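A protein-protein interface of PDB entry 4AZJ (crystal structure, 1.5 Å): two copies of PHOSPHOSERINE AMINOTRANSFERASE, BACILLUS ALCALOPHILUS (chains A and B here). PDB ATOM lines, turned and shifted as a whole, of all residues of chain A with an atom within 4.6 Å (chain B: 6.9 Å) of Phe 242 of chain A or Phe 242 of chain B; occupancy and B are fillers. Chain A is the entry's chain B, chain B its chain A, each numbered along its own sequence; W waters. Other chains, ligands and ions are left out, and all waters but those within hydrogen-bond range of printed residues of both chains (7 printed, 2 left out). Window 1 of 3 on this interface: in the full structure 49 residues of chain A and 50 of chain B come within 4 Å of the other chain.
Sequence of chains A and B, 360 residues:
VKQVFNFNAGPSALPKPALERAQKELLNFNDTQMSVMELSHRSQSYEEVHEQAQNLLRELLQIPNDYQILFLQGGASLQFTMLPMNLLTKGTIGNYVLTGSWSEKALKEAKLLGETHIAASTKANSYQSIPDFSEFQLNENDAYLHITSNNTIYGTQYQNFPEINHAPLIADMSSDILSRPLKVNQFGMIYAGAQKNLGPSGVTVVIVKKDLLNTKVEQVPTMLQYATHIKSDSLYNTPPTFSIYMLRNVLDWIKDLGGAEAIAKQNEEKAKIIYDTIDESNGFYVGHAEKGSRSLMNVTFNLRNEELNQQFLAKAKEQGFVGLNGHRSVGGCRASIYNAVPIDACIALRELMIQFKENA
Of the printed residues of chain B, Phe 242 of chain A touches Met 37 (3.8 Å) and Phe 242 (3.3 Å).
Of chain A, only Met 37 (3.9 Å) and Phe 242 (3.3 Å) come within 4 Å of Phe 242 of chain B.
Of the printed residues of chain A, Met 37 of chain B touches Phe 242 (3.8 Å).
Of the printed residues of chain A, Gln 23 of chain B touches Leu 26 (3.6 Å).
The nearest printed residue of chain A that does not touch Pro 240 of chain B is Ser 243 of chain A (6.1 Å).
The side-chain hydroxyl of Ser 201 of chain B is in hydrogen-bond range of the backbone NH of Thr 241 of chain A (3.1 Å).
OG of Ser 201 of chain A lies within hydrogen-bond range of O of Pro 239 of chain B, at 3.0 Å.
The side-chain hydroxyl (OG) of Ser 201 of chain A is in hydrogen-bond range of the backbone NH (N) of Thr 241 of chain B, at 3.1 Å.
Among the printed residues, merely in contact across the chains: Leu 26 of chain A with Ala 22 of chain B (3.95 Å), Leu 26 of chain A with Gln 23 of chain B (3.6 Å), Met 37 of chain A with Phe 242 of chain B (3.9 Å), Ser 201 of chain A with Pro 240 of chain B (3.7 Å), Pro 240 of chain A with Ser 201 of chain B (3.8 Å), Phe 242 of chain A with Met 37 of chain B (3.8 Å) and Phe 242 of chain A with Phe 242 of chain B (3.3 Å).
Of the 11 printed residues of chain A, 6 touch a printed residue of chain B.
Hydrophobic or aromatic side chains of chain B that line the printed part of chain A: Ala 22, Met 37 and Phe 242.
Among the printed residues, 10 pairs touch across the chains.
Met 37 of chain A touches Phe 242 of chain B, and with the chains exchanged Phe 242 of chain A touches Met 37 of chain B.
Ser 201 of chain A touches Pro 240 of chain B, and with the chains exchanged Pro 240 of chain A touches Ser 201 of chain B.
Ser 201 of chain A touches Thr 241 of chain B, and with the chains exchanged Thr 241 of chain A touches Ser 201 of chain B.
Phe 242 of chain A touches its own counterpart, Phe 242 of chain B.
Positions printed for both chains: 26, 36, 37, 201, 240, 241, 242, 243, 244, 245 and 246.
The side-chain hydroxyl (OG) of Ser 35 of chain B sits close to the backbone NH (N) of Met 37 of chain B.
O of Ser 201 of chain B lies within hydrogen-bond range of OG of Ser 243 of chain B (2.8 Å).
O of Ser 201 of chain A lies within hydrogen-bond range of OG of Ser 243 of chain A.
Water W4 lies within hydrogen-bond range of the side-chain hydroxyl (OG) of Ser 201 of chain A (2.9 Å), the backbone NH (N) of Phe 242 of chain B (3.1 Å) and the side-chain hydroxyl (OG1) of Thr 241 of chain B (3.3 Å).
Water W6 lies within hydrogen-bond range of the side-chain hydroxyl (OG) of Ser 201 of chain B (2.9 Å), the backbone NH (N) of Phe 242 of chain A (3.2 Å) and the side-chain hydroxyl (OG1) of Thr 241 of chain A (3.5 Å).
Water W2 lies within hydrogen-bond range of O of Met 37 of chain B, N of Ser 201 of chain A and OG1 of Thr 241 of chain B.
Water W7 bridges OG of Ser 243 of chain A (3.0 Å) and OG of Ser 243 of chain B (3.1 Å).
Water W5 lies within hydrogen-bond range of the backbone NH (N) of Ser 243 of chain A, the backbone NH (N) of Phe 242 of chain A, the backbone carbonyl oxygen (O) of Pro 240 of chain A and the backbone carbonyl oxygen (O) of Ser 201 of chain B.
Water W1 bridges N of Leu 26 of chain A (3.3 Å) and NE2 of Gln 23 of chain B (3.4 Å).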
ATOM      1  N   LEU A  26     -18.427   9.890  -8.563  1.00  0.00           N
ATOM      2  CA  LEU A  26     -19.486   8.878  -8.736  1.00  0.00           C
ATOM      3  C   LEU A  26     -19.804   8.145  -7.437  1.00  0.00           C
ATOM      4  O   LEU A  26     -20.940   7.721  -7.232  1.00  0.00           O
ATOM      5  CB  LEU A  26     -19.135   7.887  -9.852  1.00  0.00           C
ATOM      6  CG  LEU A  26     -20.349   7.169 -10.422  1.00  0.00           C
ATOM      7  CD1 LEU A  26     -21.166   8.131 -11.307  1.00  0.00           C
ATOM      8  CD2 LEU A  26     -19.996   5.950 -11.224  1.00  0.00           C
ATOM      9  N   VAL A  36     -24.596  10.231  -6.362  1.00  0.00           N
ATOM     10  CA  VAL A  36     -25.812  10.992  -6.667  1.00  0.00           C
ATOM     11  C   VAL A  36     -26.955  10.025  -7.005  1.00  0.00           C
ATOM     12  O   VAL A  36     -28.126  10.333  -6.744  1.00  0.00           O
ATOM     13  CB  VAL A  36     -25.517  12.046  -7.775  1.00  0.00           C
ATOM     14  CG1 VAL A  36     -25.342  11.364  -9.075  1.00  0.00           C
ATOM     15  CG2 VAL A  36     -26.640  13.077  -7.826  1.00  0.00           C
ATOM     16  N   MET A  37     -26.623   8.842  -7.509  1.00  0.00           N
ATOM     17  CA  MET A  37     -27.594   7.809  -7.895  1.00  0.00           C
ATOM     18  C   MET A  37     -28.269   7.143  -6.709  1.00  0.00           C
ATOM     19  O   MET A  37     -29.230   6.388  -6.889  1.00  0.00           O
ATOM     20  CB  MET A  37     -26.907   6.661  -8.677  1.00  0.00           C
ATOM     21  CG  MET A  37     -26.805   6.936 -10.119  1.00  0.00           C
ATOM     22  SD  MET A  37     -25.946   5.522 -10.863  1.00  0.00           S
ATOM     23  CE  MET A  37     -24.322   6.172 -10.955  1.00  0.00           C
ATOM     24  N   SER A 201     -29.343  10.135 -22.246  1.00  0.00           N
ATOM     25  CA  SER A 201     -30.706   9.767 -22.450  1.00  0.00           C
ATOM     26  C   SER A 201     -31.398   9.553 -21.123  1.00  0.00           C
ATOM     27  O   SER A 201     -30.747   9.389 -20.077  1.00  0.00           O
ATOM     28  CB  SER A 201     -30.744   8.488 -23.282  1.00  0.00           C
ATOM     29  OG  SER A 201     -30.209   7.426 -22.542  1.00  0.00           O
ATOM     30  N   PRO A 240     -35.576  11.011 -13.190  1.00  0.00           N
ATOM     31  CA  PRO A 240     -34.344  10.347 -13.612  1.00  0.00           C
ATOM     32  C   PRO A 240     -33.150  11.104 -13.054  1.00  0.00           C
ATOM     33  O   PRO A 240     -32.584  11.981 -13.684  1.00  0.00           O
ATOM     34  CB  PRO A 240     -34.417  10.402 -15.134  1.00  0.00           C
ATOM     35  CG  PRO A 240     -35.225  11.663 -15.406  1.00  0.00           C
ATOM     36  CD  PRO A 240     -36.230  11.748 -14.288  1.00  0.00           C
ATOM     37  N   THR A 241     -32.830  10.795 -11.805  1.00  0.00           N
ATOM     38  CA  THR A 241     -31.945  11.664 -11.052  1.00  0.00           C
ATOM     39  C   THR A 241     -30.543  11.757 -11.631  1.00  0.00           C
ATOM     40  O   THR A 241     -29.960  12.839 -11.710  1.00  0.00           O
ATOM     41  CB  THR A 241     -31.864  11.243  -9.572  1.00  0.00           C
ATOM     42  OG1 THR A 241     -31.407   9.894  -9.503  1.00  0.00           O
ATOM     43  CG2 THR A 241     -33.213  11.392  -8.861  1.00  0.00           C
ATOM     44  N   PHE A 242     -29.958  10.632 -12.048  1.00  0.00           N
ATOM     45  CA  PHE A 242     -28.636  10.694 -12.648  1.00  0.00           C
ATOM     46  C   PHE A 242     -28.618  11.436 -13.967  1.00  0.00           C
ATOM     47  O   PHE A 242     -27.695  12.162 -14.258  1.00  0.00           O
ATOM     48  CB  PHE A 242     -28.012   9.282 -12.820  1.00  0.00           C
ATOM     49  CG  PHE A 242     -26.557   9.321 -13.209  1.00  0.00           C
ATOM     50  CD1 PHE A 242     -25.598   9.742 -12.283  1.00  0.00           C
ATOM     51  CD2 PHE A 242     -26.132   8.984 -14.471  1.00  0.00           C
ATOM     52  CE1 PHE A 242     -24.244   9.811 -12.655  1.00  0.00           C
ATOM     53  CE2 PHE A 242     -24.801   9.058 -14.820  1.00  0.00           C
ATOM     54  CZ  PHE A 242     -23.865   9.478 -13.899  1.00  0.00           C
ATOM     55  N   SER A 243     -29.657  11.241 -14.780  1.00  0.00           N
ATOM     56  CA  SER A 243     -29.718  11.983 -16.028  1.00  0.00           C
ATOM     57  C   SER A 243     -29.770  13.473 -15.746  1.00  0.00           C
ATOM     58  O   SER A 243     -29.140  14.234 -16.450  1.00  0.00           O
ATOM     59  CB  SER A 243     -30.923  11.562 -16.860  1.00  0.00           C
ATOM     60  OG  SER A 243     -30.737  10.233 -17.321  1.00  0.00           O
ATOM     61  N   ILE A 244     -30.525  13.885 -14.728  1.00  0.00           N
ATOM     62  CA  ILE A 244     -30.634  15.316 -14.432  1.00  0.00           C
ATOM     63  C   ILE A 244     -29.306  15.855 -13.902  1.00  0.00           C
ATOM     64  O   ILE A 244     -28.884  16.992 -14.212  1.00  0.00           O
ATOM     65  CB  ILE A 244     -31.827  15.588 -13.522  1.00  0.00           C
ATOM     66  CG1 ILE A 244     -33.156  15.314 -14.285  1.00  0.00           C
ATOM     67  CG2 ILE A 244     -31.775  17.017 -12.923  1.00  0.00           C
ATOM     68  CD1 ILE A 244     -34.412  15.148 -13.445  1.00  0.00           C
ATOM     69  N   TYR A 245     -28.633  15.048 -13.095  1.00  0.00           N
ATOM     70  CA  TYR A 245     -27.283  15.388 -12.637  1.00  0.00           C
ATOM     71  C   TYR A 245     -26.345  15.582 -13.834  1.00  0.00           C
ATOM     72  O   TYR A 245     -25.585  16.546 -13.899  1.00  0.00           O
ATOM     73  CB  TYR A 245     -26.761  14.308 -11.642  1.00  0.00           C
ATOM     74  CG  TYR A 245     -25.268  14.343 -11.460  1.00  0.00           C
ATOM     75  CD1 TYR A 245     -24.675  15.185 -10.528  1.00  0.00           C
ATOM     76  CD2 TYR A 245     -24.455  13.552 -12.229  1.00  0.00           C
ATOM     77  CE1 TYR A 245     -23.316  15.238 -10.388  1.00  0.00           C
ATOM     78  CE2 TYR A 245     -23.107  13.596 -12.114  1.00  0.00           C
ATOM     79  CZ  TYR A 245     -22.536  14.441 -11.192  1.00  0.00           C
ATOM     80  OH  TYR A 245     -21.156  14.480 -11.076  1.00  0.00           O
ATOM     81  N   MET A 246     -26.365  14.652 -14.785  1.00  0.00           N
ATOM     82  CA  MET A 246     -25.498  14.793 -15.930  1.00  0.00           C
ATOM     83  C   MET A 246     -25.835  16.012 -16.775  1.00  0.00           C
ATOM     84  O   MET A 246     -24.942  16.652 -17.304  1.00  0.00           O
ATOM     85  CB  MET A 246     -25.558  13.540 -16.808  1.00  0.00           C
ATOM     86  CG  MET A 246     -24.846  12.326 -16.247  1.00  0.00           C
ATOM     87  SD  MET A 246     -23.084  12.561 -15.905  1.00  0.00           S
ATOM     88  CE  MET A 246     -22.490  13.225 -17.416  1.00  0.00           C
ATOM     89  N   ALA B  22     -18.872   0.868 -12.694  1.00  0.00           N
ATOM     90  CA  ALA B  22     -19.337   1.987 -13.515  1.00  0.00           C
ATOM     91  C   ALA B  22     -18.325   3.107 -13.538  1.00  0.00           C
ATOM     92  O   ALA B  22     -18.026   3.702 -14.589  1.00  0.00           O
ATOM     93  CB  ALA B  22     -20.651   2.484 -13.006  1.00  0.00           C
ATOM     94  N   GLN B  23     -17.770   3.420 -12.373  1.00  0.00           N
ATOM     95  CA  GLN B  23     -16.798   4.490 -12.293  1.00  0.00           C
ATOM     96  C   GLN B  23     -15.575   4.193 -13.146  1.00  0.00           C
ATOM     97  O   GLN B  23     -15.100   5.052 -13.885  1.00  0.00           O
ATOM     98  CB  GLN B  23     -16.363   4.706 -10.845  1.00  0.00           C
ATOM     99  CG  GLN B  23     -15.389   5.855 -10.668  1.00  0.00           C
ATOM    100  CD  GLN B  23     -14.929   6.003  -9.236  1.00  0.00           C
ATOM    101  OE1 GLN B  23     -14.535   5.017  -8.605  1.00  0.00           O
ATOM    102  NE2 GLN B  23     -15.021   7.201  -8.701  1.00  0.00           N
ATOM    103  N   LEU B  26     -16.321   4.558 -16.917  1.00  0.00           N
ATOM    104  CA  LEU B  26     -17.243   5.628 -17.317  1.00  0.00           C
ATOM    105  C   LEU B  26     -16.802   6.368 -18.586  1.00  0.00           C
ATOM    106  O   LEU B  26     -17.661   6.865 -19.326  1.00  0.00           O
ATOM    107  CB  LEU B  26     -17.436   6.626 -16.191  1.00  0.00           C
ATOM    108  CG  LEU B  26     -18.752   7.416 -16.298  1.00  0.00           C
ATOM    109  CD1 LEU B  26     -19.938   6.511 -15.948  1.00  0.00           C
ATOM    110  CD2 LEU B  26     -18.699   8.668 -15.402  1.00  0.00           C
ATOM    111  N   SER B  35     -17.915   6.530 -23.432  1.00  0.00           N
ATOM    112  CA  SER B  35     -18.774   6.130 -22.323  1.00  0.00           C
ATOM    113  C   SER B  35     -19.966   5.320 -22.819  1.00  0.00           C
ATOM    114  O   SER B  35     -20.432   5.510 -23.939  1.00  0.00           O
ATOM    115  CB  SER B  35     -19.304   7.376 -21.620  1.00  0.00           C
ATOM    116  OG  SER B  35     -20.137   7.069 -20.500  1.00  0.00           O
ATOM    117  N   VAL B  36     -20.521   4.468 -21.972  1.00  0.00           N
ATOM    118  CA  VAL B  36     -21.789   3.849 -22.293  1.00  0.00           C
ATOM    119  C   VAL B  36     -22.811   4.903 -22.613  1.00  0.00           C
ATOM    120  O   VAL B  36     -23.690   4.677 -23.471  1.00  0.00           O
ATOM    121  CB  VAL B  36     -22.367   3.059 -21.092  1.00  0.00           C
ATOM    122  CG1 VAL B  36     -23.901   2.916 -21.216  1.00  0.00           C
ATOM    123  CG2 VAL B  36     -21.720   1.739 -20.999  1.00  0.00           C
ATOM    124  N   MET B  37     -22.683   6.077 -21.977  1.00  0.00           N
ATOM    125  CA  MET B  37     -23.610   7.220 -22.168  1.00  0.00           C
ATOM    126  C   MET B  37     -23.521   7.876 -23.548  1.00  0.00           C
ATOM    127  O   MET B  37     -24.329   8.764 -23.883  1.00  0.00           O
ATOM    128  CB  MET B  37     -23.310   8.355 -21.155  1.00  0.00           C
ATOM    129  CG  MET B  37     -23.917   8.038 -19.847  1.00  0.00           C
ATOM    130  SD  MET B  37     -23.628   9.407 -18.725  1.00  0.00           S
ATOM    131  CE  MET B  37     -22.375   8.673 -17.739  1.00  0.00           C
ATOM    132  N   TYR B  46     -24.199  -1.077 -27.591  1.00  0.00           N
ATOM    133  CA  TYR B  46     -25.317  -0.893 -26.678  1.00  0.00           C
ATOM    134  C   TYR B  46     -26.259  -2.106 -26.658  1.00  0.00           C
ATOM    135  O   TYR B  46     -26.699  -2.564 -25.583  1.00  0.00           O
ATOM    136  CB  TYR B  46     -26.118   0.429 -26.918  1.00  0.00           C
ATOM    137  CG  TYR B  46     -27.269   0.412 -25.973  1.00  0.00           C
ATOM    138  CD1 TYR B  46     -27.057   0.637 -24.613  1.00  0.00           C
ATOM    139  CD2 TYR B  46     -28.539   0.048 -26.405  1.00  0.00           C
ATOM    140  CE1 TYR B  46     -28.082   0.472 -23.705  1.00  0.00           C
ATOM    141  CE2 TYR B  46     -29.581  -0.112 -25.503  1.00  0.00           C
ATOM    142  CZ  TYR B  46     -29.335   0.109 -24.159  1.00  0.00           C
ATOM    143  OH  TYR B  46     -30.364  -0.059 -23.268  1.00  0.00           O
ATOM    144  N   PRO B 200     -30.772   2.130 -10.723  1.00  0.00           N
ATOM    145  CA  PRO B 200     -30.993   3.519 -10.430  1.00  0.00           C
ATOM    146  C   PRO B 200     -32.333   3.890 -11.005  1.00  0.00           C
ATOM    147  O   PRO B 200     -33.046   3.062 -11.560  1.00  0.00           O
ATOM    148  CB  PRO B 200     -29.840   4.215 -11.166  1.00  0.00           C
ATOM    149  CG  PRO B 200     -29.689   3.360 -12.413  1.00  0.00           C
ATOM    150  CD  PRO B 200     -30.143   1.938 -12.039  1.00  0.00           C
ATOM    151  N   SER B 201     -32.734   5.129 -10.798  1.00  0.00           N
ATOM    152  CA  SER B 201     -33.984   5.582 -11.338  1.00  0.00           C
ATOM    153  C   SER B 201     -33.815   5.810 -12.819  1.00  0.00           C
ATOM    154  O   SER B 201     -32.690   5.802 -13.364  1.00  0.00           O
ATOM    155  CB  SER B 201     -34.430   6.876 -10.671  1.00  0.00           C
ATOM    156  OG  SER B 201     -33.453   7.864 -10.861  1.00  0.00           O
ATOM    157  N   PRO B 239     -33.852   4.359 -25.414  1.00  0.00           N
ATOM    158  CA  PRO B 239     -34.000   3.889 -24.041  1.00  0.00           C
ATOM    159  C   PRO B 239     -33.109   4.679 -23.115  1.00  0.00           C
ATOM    160  O   PRO B 239     -32.195   5.379 -23.565  1.00  0.00           O
ATOM    161  CB  PRO B 239     -33.516   2.444 -24.110  1.00  0.00           C
ATOM    162  CG  PRO B 239     -32.589   2.389 -25.268  1.00  0.00           C
ATOM    163  CD  PRO B 239     -33.027   3.463 -26.225  1.00  0.00           C
ATOM    164  N   PRO B 240     -33.346   4.530 -21.801  1.00  0.00           N
ATOM    165  CA  PRO B 240     -32.455   5.122 -20.786  1.00  0.00           C
ATOM    166  C   PRO B 240     -31.215   4.251 -20.657  1.00  0.00           C
ATOM    167  O   PRO B 240     -31.114   3.378 -19.786  1.00  0.00           O
ATOM    168  CB  PRO B 240     -33.313   5.102 -19.506  1.00  0.00           C
ATOM    169  CG  PRO B 240     -34.229   3.910 -19.714  1.00  0.00           C
ATOM    170  CD  PRO B 240     -34.528   3.893 -21.197  1.00  0.00           C
ATOM    171  N   THR B 241     -30.273   4.474 -21.571  1.00  0.00           N
ATOM    172  CA  THR B 241     -29.175   3.562 -21.769  1.00  0.00           C
ATOM    173  C   THR B 241     -28.302   3.413 -20.531  1.00  0.00           C
ATOM    174  O   THR B 241     -27.883   2.305 -20.195  1.00  0.00           O
ATOM    175  CB  THR B 241     -28.293   3.980 -22.945  1.00  0.00           C
ATOM    176  OG1 THR B 241     -27.865   5.329 -22.775  1.00  0.00           O
ATOM    177  CG2 THR B 241     -29.070   3.890 -24.230  1.00  0.00           C
ATOM    178  N   PHE B 242     -28.007   4.491 -19.829  1.00  0.00           N
ATOM    179  CA  PHE B 242     -27.146   4.368 -18.646  1.00  0.00           C
ATOM    180  C   PHE B 242     -27.877   3.665 -17.517  1.00  0.00           C
ATOM    181  O   PHE B 242     -27.291   2.876 -16.793  1.00  0.00           O
ATOM    182  CB  PHE B 242     -26.587   5.716 -18.164  1.00  0.00           C
ATOM    183  CG  PHE B 242     -25.525   5.575 -17.113  1.00  0.00           C
ATOM    184  CD1 PHE B 242     -24.272   5.119 -17.461  1.00  0.00           C
ATOM    185  CD2 PHE B 242     -25.795   5.876 -15.810  1.00  0.00           C
ATOM    186  CE1 PHE B 242     -23.282   4.959 -16.486  1.00  0.00           C
ATOM    187  CE2 PHE B 242     -24.777   5.728 -14.828  1.00  0.00           C
ATOM    188  CZ  PHE B 242     -23.532   5.271 -15.214  1.00  0.00           C
ATOM    189  N   SER B 243     -29.170   3.917 -17.376  1.00  0.00           N
ATOM    190  CA  SER B 243     -29.936   3.220 -16.348  1.00  0.00           C
ATOM    191  C   SER B 243     -29.936   1.714 -16.613  1.00  0.00           C
ATOM    192  O   SER B 243     -29.835   0.925 -15.678  1.00  0.00           O
ATOM    193  CB  SER B 243     -31.360   3.733 -16.280  1.00  0.00           C
ATOM    194  OG  SER B 243     -31.350   5.063 -15.760  1.00  0.00           O
ATOM    195  N   ILE B 244     -30.061   1.310 -17.874  1.00  0.00           N
ATOM    196  CA  ILE B 244     -30.090  -0.100 -18.219  1.00  0.00           C
ATOM    197  C   ILE B 244     -28.714  -0.720 -17.989  1.00  0.00           C
ATOM    198  O   ILE B 244     -28.593  -1.844 -17.533  1.00  0.00           O
ATOM    199  CB  ILE B 244     -30.633  -0.274 -19.643  1.00  0.00           C
ATOM    200  CG1 ILE B 244     -32.120   0.084 -19.636  1.00  0.00           C
ATOM    201  CG2 ILE B 244     -30.418  -1.700 -20.142  1.00  0.00           C
ATOM    202  CD1 ILE B 244     -32.739   0.322 -21.034  1.00  0.00           C
ATOM    203  N   TYR B 245     -27.683   0.023 -18.327  1.00  0.00           N
ATOM    204  CA  TYR B 245     -26.325  -0.384 -18.007  1.00  0.00           C
ATOM    205  C   TYR B 245     -26.138  -0.594 -16.509  1.00  0.00           C
ATOM    206  O   TYR B 245     -25.567  -1.605 -16.082  1.00  0.00           O
ATOM    207  CB  TYR B 245     -25.307   0.622 -18.591  1.00  0.00           C
ATOM    208  CG  TYR B 245     -23.948   0.529 -17.984  1.00  0.00           C
ATOM    209  CD1 TYR B 245     -23.640   1.255 -16.867  1.00  0.00           C
ATOM    210  CD2 TYR B 245     -22.991  -0.326 -18.497  1.00  0.00           C
ATOM    211  CE1 TYR B 245     -22.394   1.162 -16.282  1.00  0.00           C
ATOM    212  CE2 TYR B 245     -21.744  -0.433 -17.899  1.00  0.00           C
ATOM    213  CZ  TYR B 245     -21.467   0.296 -16.819  1.00  0.00           C
ATOM    214  OH  TYR B 245     -20.225   0.178 -16.225  1.00  0.00           O
ATOM    215  N   MET B 246     -26.594   0.349 -15.688  1.00  0.00           N
ATOM    216  CA  MET B 246     -26.444   0.193 -14.256  1.00  0.00           C
ATOM    217  C   MET B 246     -27.259  -0.994 -13.750  1.00  0.00           C
ATOM    218  O   MET B 246     -26.814  -1.714 -12.850  1.00  0.00           O
ATOM    219  CB  MET B 246     -26.857   1.474 -13.516  1.00  0.00           C
ATOM    220  CG  MET B 246     -25.894   2.603 -13.652  1.00  0.00           C
ATOM    221  SD  MET B 246     -24.257   2.230 -12.973  1.00  0.00           S
ATOM    222  CE  MET B 246     -24.653   1.582 -11.368  1.00  0.00           C
ATOM    223  N   LEU B 247     -28.442  -1.211 -14.313  1.00  0.00           N
ATOM    224  CA  LEU B 247     -29.248  -2.405 -14.005  1.00  0.00           C
ATOM    225  C   LEU B 247     -28.447  -3.672 -14.290  1.00  0.00           C
ATOM    226  O   LEU B 247     -28.394  -4.585 -13.475  1.00  0.00           O
ATOM    227  CB  LEU B 247     -30.542  -2.393 -14.826  1.00  0.00           C
ATOM    228  CG  LEU B 247     -31.419  -3.655 -14.849  1.00  0.00           C
ATOM    229  CD1 LEU B 247     -32.067  -3.851 -13.494  1.00  0.00           C
ATOM    230  CD2 LEU B 247     -32.488  -3.596 -15.935  1.00  0.00           C
ATOM    231  N   ARG B 248     -27.816  -3.740 -15.459  1.00  0.00           N
ATOM    232  CA  ARG B 248     -26.949  -4.869 -15.764  1.00  0.00           C
ATOM    233  C   ARG B 248     -25.905  -5.057 -14.651  1.00  0.00           C
ATOM    234  O   ARG B 248     -25.699  -6.175 -14.153  1.00  0.00           O
ATOM    235  CB  ARG B 248     -26.286  -4.623 -17.115  1.00  0.00           C
ATOM    236  CG  ARG B 248     -25.517  -5.800 -17.713  1.00  0.00           C
ATOM    237  CD  ARG B 248     -24.229  -6.106 -17.084  1.00  0.00           C
ATOM    238  NE  ARG B 248     -23.275  -4.999 -17.076  1.00  0.00           N
ATOM    239  CZ  ARG B 248     -22.327  -4.746 -17.982  1.00  0.00           C
ATOM    240  NH1 ARG B 248     -22.144  -5.486 -19.088  1.00  0.00           N
ATOM    241  NH2 ARG B 248     -21.504  -3.753 -17.781  1.00  0.00           N
HETATM  242  O   HOH W   1     -16.233   9.202  -6.168  1.00  0.00           O
HETATM  243  O   HOH W   2     -27.111   8.279 -22.972  1.00  0.00           O
HETATM  244  O   HOH W   3     -30.284   6.471 -18.646  1.00  0.00           O
HETATM  245  O   HOH W   4     -28.369   7.492 -20.337  1.00  0.00           O
HETATM  246  O   HOH W   5     -31.481   8.842 -14.418  1.00  0.00           O
HETATM  247  O   HOH W   6     -30.754   7.576 -12.007  1.00  0.00           O
HETATM  248  O   HOH W   7     -32.351   7.713 -16.922  1.00  0.00           O
